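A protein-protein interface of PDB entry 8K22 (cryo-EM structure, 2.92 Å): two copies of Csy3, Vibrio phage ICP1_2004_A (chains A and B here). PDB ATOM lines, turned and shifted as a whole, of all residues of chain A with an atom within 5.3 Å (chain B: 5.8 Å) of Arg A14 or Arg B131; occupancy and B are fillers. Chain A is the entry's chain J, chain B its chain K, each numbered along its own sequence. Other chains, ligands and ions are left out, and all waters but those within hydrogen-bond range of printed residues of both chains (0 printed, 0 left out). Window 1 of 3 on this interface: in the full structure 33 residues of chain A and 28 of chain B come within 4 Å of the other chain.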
ATOM      1  N   TYR A  12      20.244  22.300  25.724  1.00  0.00           N
ATOM      2  CA  TYR A  12      18.836  22.580  25.500  1.00  0.00           C
ATOM      3  C   TYR A  12      18.589  22.746  24.010  1.00  0.00           C
ATOM      4  O   TYR A  12      19.348  23.429  23.319  1.00  0.00           O
ATOM      5  CB  TYR A  12      18.402  23.840  26.241  1.00  0.00           C
ATOM      6  CG  TYR A  12      18.064  23.616  27.693  1.00  0.00           C
ATOM      7  CD1 TYR A  12      19.063  23.506  28.646  1.00  0.00           C
ATOM      8  CD2 TYR A  12      16.747  23.530  28.110  1.00  0.00           C
ATOM      9  CE1 TYR A  12      18.764  23.318  29.971  1.00  0.00           C
ATOM     10  CE2 TYR A  12      16.435  23.335  29.439  1.00  0.00           C
ATOM     11  CZ  TYR A  12      17.451  23.226  30.364  1.00  0.00           C
ATOM     12  OH  TYR A  12      17.154  23.031  31.690  1.00  0.00           O
ATOM     13  N   SER A  13      17.535  22.106  23.517  1.00  0.00           N
ATOM     14  CA  SER A  13      17.155  22.266  22.126  1.00  0.00           C
ATOM     15  C   SER A  13      16.532  23.638  21.905  1.00  0.00           C
ATOM     16  O   SER A  13      16.020  24.273  22.830  1.00  0.00           O
ATOM     17  CB  SER A  13      16.176  21.176  21.702  1.00  0.00           C
ATOM     18  OG  SER A  13      15.391  21.603  20.604  1.00  0.00           O
ATOM     19  N   ARG A  14      16.592  24.097  20.661  1.00  0.00           N
ATOM     20  CA  ARG A  14      15.979  25.367  20.314  1.00  0.00           C
ATOM     21  C   ARG A  14      14.460  25.229  20.310  1.00  0.00           C
ATOM     22  O   ARG A  14      13.908  24.157  20.047  1.00  0.00           O
ATOM     23  CB  ARG A  14      16.510  25.862  18.963  1.00  0.00           C
ATOM     24  CG  ARG A  14      15.720  25.454  17.737  1.00  0.00           C
ATOM     25  CD  ARG A  14      16.090  26.306  16.542  1.00  0.00           C
ATOM     26  NE  ARG A  14      17.404  25.975  16.011  1.00  0.00           N
ATOM     27  CZ  ARG A  14      17.615  25.089  15.050  1.00  0.00           C
ATOM     28  NH1 ARG A  14      16.617  24.420  14.497  1.00  0.00           N
ATOM     29  NH2 ARG A  14      18.857  24.865  14.633  1.00  0.00           N
ATOM     30  N   LYS A  15      13.784  26.315  20.678  1.00  0.00           N
ATOM     31  CA  LYS A  15      12.334  26.322  20.743  1.00  0.00           C
ATOM     32  C   LYS A  15      11.687  27.275  19.756  1.00  0.00           C
ATOM     33  O   LYS A  15      10.501  27.107  19.456  1.00  0.00           O
ATOM     34  CB  LYS A  15      11.860  26.672  22.161  1.00  0.00           C
ATOM     35  CG  LYS A  15      12.263  25.654  23.213  1.00  0.00           C
ATOM     36  CD  LYS A  15      11.932  24.233  22.788  1.00  0.00           C
ATOM     37  CE  LYS A  15      12.599  23.218  23.696  1.00  0.00           C
ATOM     38  NZ  LYS A  15      13.929  23.685  24.164  1.00  0.00           N
ATOM     39  N   ILE A  16      12.415  28.266  19.262  1.00  0.00           N
ATOM     40  CA  ILE A  16      11.971  29.097  18.152  1.00  0.00           C
ATOM     41  C   ILE A  16      12.639  28.560  16.899  1.00  0.00           C
ATOM     42  O   ILE A  16      13.860  28.667  16.748  1.00  0.00           O
ATOM     43  CB  ILE A  16      12.334  30.571  18.369  1.00  0.00           C
ATOM     44  CG1 ILE A  16      11.663  31.102  19.624  1.00  0.00           C
ATOM     45  CG2 ILE A  16      11.921  31.394  17.168  1.00  0.00           C
ATOM     46  CD1 ILE A  16      12.216  32.416  20.076  1.00  0.00           C
ATOM     47  N   ASN A  17      11.843  27.993  15.993  1.00  0.00           N
ATOM     48  CA  ASN A  17      12.339  27.349  14.783  1.00  0.00           C
ATOM     49  C   ASN A  17      11.756  28.087  13.586  1.00  0.00           C
ATOM     50  O   ASN A  17      10.660  27.754  13.117  1.00  0.00           O
ATOM     51  CB  ASN A  17      11.953  25.872  14.741  1.00  0.00           C
ATOM     52  CG  ASN A  17      12.705  25.041  15.753  1.00  0.00           C
ATOM     53  OD1 ASN A  17      13.639  24.320  15.406  1.00  0.00           O
ATOM     54  ND2 ASN A  17      12.295  25.125  17.011  1.00  0.00           N
ATOM     55  N   PRO A  18      12.428  29.119  13.093  1.00  0.00           N
ATOM     56  CA  PRO A  18      12.003  29.728  11.836  1.00  0.00           C
ATOM     57  C   PRO A  18      12.511  28.919  10.656  1.00  0.00           C
ATOM     58  O   PRO A  18      13.490  28.179  10.746  1.00  0.00           O
ATOM     59  CB  PRO A  18      12.643  31.118  11.878  1.00  0.00           C
ATOM     60  CG  PRO A  18      13.812  30.963  12.752  1.00  0.00           C
ATOM     61  CD  PRO A  18      13.569  29.827  13.693  1.00  0.00           C
ATOM     62  N   VAL A  86       7.986  26.087  19.790  1.00  0.00           N
ATOM     63  CA  VAL A  86       7.690  24.814  20.432  1.00  0.00           C
ATOM     64  C   VAL A  86       7.724  24.999  21.942  1.00  0.00           C
ATOM     65  O   VAL A  86       8.412  25.887  22.439  1.00  0.00           O
ATOM     66  CB  VAL A  86       8.679  23.710  20.003  1.00  0.00           C
ATOM     67  CG1 VAL A  86       7.997  22.352  20.013  1.00  0.00           C
ATOM     68  CG2 VAL A  86       9.226  23.993  18.613  1.00  0.00           C
ATOM     69  N   ILE A 296      14.835  28.971  25.698  1.00  0.00           N
ATOM     70  CA  ILE A 296      14.019  28.981  24.489  1.00  0.00           C
ATOM     71  C   ILE A 296      14.907  29.042  23.251  1.00  0.00           C
ATOM     72  O   ILE A 296      14.665  28.341  22.259  1.00  0.00           O
ATOM     73  CB  ILE A 296      13.017  30.150  24.554  1.00  0.00           C
ATOM     74  CG1 ILE A 296      11.914  29.847  25.564  1.00  0.00           C
ATOM     75  CG2 ILE A 296      12.376  30.414  23.216  1.00  0.00           C
ATOM     76  CD1 ILE A 296      11.180  31.076  26.036  1.00  0.00           C
ATOM     77  N   ARG A 297      15.960  29.864  23.296  1.00  0.00           N
ATOM     78  CA  ARG A 297      16.959  29.877  22.231  1.00  0.00           C
ATOM     79  C   ARG A 297      17.676  28.539  22.139  1.00  0.00           C
ATOM     80  O   ARG A 297      17.911  28.021  21.041  1.00  0.00           O
ATOM     81  CB  ARG A 297      17.965  31.005  22.476  1.00  0.00           C
ATOM     82  CG  ARG A 297      19.315  30.829  21.790  1.00  0.00           C
ATOM     83  CD  ARG A 297      20.451  31.226  22.707  1.00  0.00           C
ATOM     84  NE  ARG A 297      21.725  31.304  22.004  1.00  0.00           N
ATOM     85  CZ  ARG A 297      22.647  30.352  22.021  1.00  0.00           C
ATOM     86  NH1 ARG A 297      22.465  29.228  22.693  1.00  0.00           N
ATOM     87  NH2 ARG A 297      23.778  30.533  21.349  1.00  0.00           N
ATOM     88  N   GLY A 298      17.991  27.948  23.276  1.00  0.00           N
ATOM     89  CA  GLY A 298      18.707  26.697  23.302  1.00  0.00           C
ATOM     90  C   GLY A 298      20.183  26.913  23.534  1.00  0.00           C
ATOM     91  O   GLY A 298      20.639  27.969  23.978  1.00  0.00           O
ATOM     92  N   LEU B 129      10.878   9.504  16.053  1.00  0.00           N
ATOM     93  CA  LEU B 129      10.897  10.780  15.350  1.00  0.00           C
ATOM     94  C   LEU B 129      11.087  11.931  16.332  1.00  0.00           C
ATOM     95  O   LEU B 129      10.289  12.867  16.339  1.00  0.00           O
ATOM     96  CB  LEU B 129       9.606  10.993  14.558  1.00  0.00           C
ATOM     97  CG  LEU B 129       8.868   9.820  13.914  1.00  0.00           C
ATOM     98  CD1 LEU B 129       7.454  10.220  13.545  1.00  0.00           C
ATOM     99  CD2 LEU B 129       9.621   9.324  12.698  1.00  0.00           C
ATOM    100  N   TRP B 130      12.147  11.863  17.157  1.00  0.00           N
ATOM    101  CA  TRP B 130      12.284  12.618  18.413  1.00  0.00           C
ATOM    102  C   TRP B 130      12.050  14.118  18.269  1.00  0.00           C
ATOM    103  O   TRP B 130      11.107  14.671  18.846  1.00  0.00           O
ATOM    104  CB  TRP B 130      13.679  12.415  19.004  1.00  0.00           C
ATOM    105  CG  TRP B 130      13.921  11.106  19.627  1.00  0.00           C
ATOM    106  CD1 TRP B 130      13.935  10.814  20.959  1.00  0.00           C
ATOM    107  CD2 TRP B 130      14.229   9.900  18.948  1.00  0.00           C
ATOM    108  NE1 TRP B 130      14.220   9.486  21.146  1.00  0.00           N
ATOM    109  CE2 TRP B 130      14.405   8.904  19.922  1.00  0.00           C
ATOM    110  CE3 TRP B 130      14.370   9.561  17.603  1.00  0.00           C
ATOM    111  CZ2 TRP B 130      14.709   7.603  19.593  1.00  0.00           C
ATOM    112  CZ3 TRP B 130      14.657   8.279  17.282  1.00  0.00           C
ATOM    113  CH2 TRP B 130      14.836   7.315  18.267  1.00  0.00           C
ATOM    114  N   ARG B 131      12.897  14.796  17.503  1.00  0.00           N
ATOM    115  CA  ARG B 131      12.813  16.243  17.440  1.00  0.00           C
ATOM    116  C   ARG B 131      11.914  16.743  16.319  1.00  0.00           C
ATOM    117  O   ARG B 131      11.643  17.946  16.256  1.00  0.00           O
ATOM    118  CB  ARG B 131      14.212  16.858  17.304  1.00  0.00           C
ATOM    119  CG  ARG B 131      14.341  18.197  18.019  1.00  0.00           C
ATOM    120  CD  ARG B 131      15.676  18.370  18.700  1.00  0.00           C
ATOM    121  NE  ARG B 131      16.656  19.005  17.831  1.00  0.00           N
ATOM    122  CZ  ARG B 131      16.776  20.316  17.670  1.00  0.00           C
ATOM    123  NH1 ARG B 131      15.959  21.164  18.272  1.00  0.00           N
ATOM    124  NH2 ARG B 131      17.741  20.788  16.888  1.00  0.00           N
ATOM    125  N   ASN B 132      11.430  15.870  15.441  1.00  0.00           N
ATOM    126  CA  ASN B 132      10.512  16.321  14.409  1.00  0.00           C
ATOM    127  C   ASN B 132       9.081  15.844  14.622  1.00  0.00           C
ATOM    128  O   ASN B 132       8.199  16.233  13.854  1.00  0.00           O
ATOM    129  CB  ASN B 132      11.018  15.921  13.016  1.00  0.00           C
ATOM    130  CG  ASN B 132      11.654  14.558  12.991  1.00  0.00           C
ATOM    131  OD1 ASN B 132      11.312  13.695  13.781  1.00  0.00           O
ATOM    132  ND2 ASN B 132      12.588  14.357  12.073  1.00  0.00           N
ATOM    133  N   ARG B 133       8.809  15.045  15.657  1.00  0.00           N
ATOM    134  CA  ARG B 133       7.417  14.858  16.046  1.00  0.00           C
ATOM    135  C   ARG B 133       6.867  16.074  16.776  1.00  0.00           C
ATOM    136  O   ARG B 133       5.645  16.254  16.815  1.00  0.00           O
ATOM    137  CB  ARG B 133       7.235  13.608  16.914  1.00  0.00           C
ATOM    138  CG  ARG B 133       7.775  13.721  18.330  1.00  0.00           C
ATOM    139  CD  ARG B 133       7.650  12.409  19.086  1.00  0.00           C
ATOM    140  NE  ARG B 133       6.435  11.678  18.743  1.00  0.00           N
ATOM    141  CZ  ARG B 133       5.241  11.910  19.275  1.00  0.00           C
ATOM    142  NH1 ARG B 133       5.062  12.849  20.189  1.00  0.00           N
ATOM    143  NH2 ARG B 133       4.203  11.180  18.879  1.00  0.00           N
ATOM    144  N   VAL B 134       7.730  16.906  17.351  1.00  0.00           N
ATOM    145  CA  VAL B 134       7.296  18.183  17.899  1.00  0.00           C
ATOM    146  C   VAL B 134       7.322  19.222  16.788  1.00  0.00           C
ATOM    147  O   VAL B 134       8.174  19.188  15.891  1.00  0.00           O
ATOM    148  CB  VAL B 134       8.158  18.590  19.111  1.00  0.00           C
ATOM    149  CG1 VAL B 134       8.016  17.560  20.220  1.00  0.00           C
ATOM    150  CG2 VAL B 134       9.622  18.742  18.739  1.00  0.00           C
ATOM    151  N   GLY B 135       6.348  20.123  16.812  1.00  0.00           N
ATOM    152  CA  GLY B 135       6.155  21.041  15.716  1.00  0.00           C
ATOM    153  C   GLY B 135       5.371  20.483  14.551  1.00  0.00           C
ATOM    154  O   GLY B 135       5.155  21.206  13.570  1.00  0.00           O
ATOM    155  N   GLU B 198      12.600  22.370   9.149  1.00  0.00           N
ATOM    156  CA  GLU B 198      13.827  21.599   9.260  1.00  0.00           C
ATOM    157  C   GLU B 198      13.526  20.236   9.866  1.00  0.00           C
ATOM    158  O   GLU B 198      12.840  20.138  10.888  1.00  0.00           O
ATOM    159  CB  GLU B 198      14.854  22.360  10.101  1.00  0.00           C
ATOM    160  CG  GLU B 198      15.822  21.501  10.899  1.00  0.00           C
ATOM    161  CD  GLU B 198      16.982  22.305  11.451  1.00  0.00           C
ATOM    162  OE1 GLU B 198      17.497  23.178  10.723  1.00  0.00           O
ATOM    163  OE2 GLU B 198      17.380  22.065  12.609  1.00  0.00           O
ATOM    164  N   PHE B 200      15.005  16.367  11.235  1.00  0.00           N
ATOM    165  CA  PHE B 200      16.056  15.989  12.175  1.00  0.00           C
ATOM    166  C   PHE B 200      16.443  14.538  11.944  1.00  0.00           C
ATOM    167  O   PHE B 200      15.872  13.622  12.553  1.00  0.00           O
ATOM    168  CB  PHE B 200      15.607  16.233  13.612  1.00  0.00           C
ATOM    169  CG  PHE B 200      15.206  17.652  13.875  1.00  0.00           C
ATOM    170  CD1 PHE B 200      16.161  18.610  14.156  1.00  0.00           C
ATOM    171  CD2 PHE B 200      13.877  18.032  13.818  1.00  0.00           C
ATOM    172  CE1 PHE B 200      15.797  19.917  14.388  1.00  0.00           C
ATOM    173  CE2 PHE B 200      13.507  19.340  14.050  1.00  0.00           C
ATOM    174  CZ  PHE B 200      14.469  20.283  14.337  1.00  0.00           C
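Arg B131 touches Arg A14 (NH1 to N, 3.8 Å). CB of Val B134 touches CG1 of Val A86, at 3.9 Å.
Of the 9 printed residues of chain B, 3 touch a printed residue of chain A. Hydrophobic or aromatic side chains of chain B that line the printed part of chain A: Val B134. Among the printed residues, Asp or Glu carboxylates within 4 Å of a Lys or Arg side-chain nitrogen of the other chain: Arg A14 with Glu B198 (3.1 Å).
O of Lys A15 lies within hydrogen-bond range of N of Val A86 (2.7 Å). The guanidinium group (NH1) of Arg A14 is in hydrogen-bond range of the side-chain amide oxygen (OD1) of Asn A17. NZ of Lys A15 lies within hydrogen-bond range of O of Ser A13 (2.5 Å).
The side-chain carboxylate (OE2) of Glu B198 lies within salt-bridge range of the guanidinium group (NH1) of Arg A14, at 3.1 Å. The guanidinium group (NH1) of Arg B131 sits at hydrogen-bond distance from the side-chain hydroxyl (OG) of Ser A13, at 2.4 Å.
Printed residues of chain B within 4 Å of Ser A13: Arg B131 (2.4 Å). Lys A15 touches none of the printed residues of chain B. Of the printed residues of chain B, Val A86 touches Val B134 (3.9 Å). Of chain A, only Ser A13 (2.4 Å) and Arg A14 (3.8 Å) come within 4 Å of Arg B131. Printed residues of chain A within 4 Å of Val B134: Val A86 (3.9 Å). Of the printed residues of chain A, Glu B198 touches Arg A14 (3.1 Å).
No position is printed for both chains. Of the 4 pairs that touch across the chains among the printed residues, none has its exchanged pair printed and touching as well.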
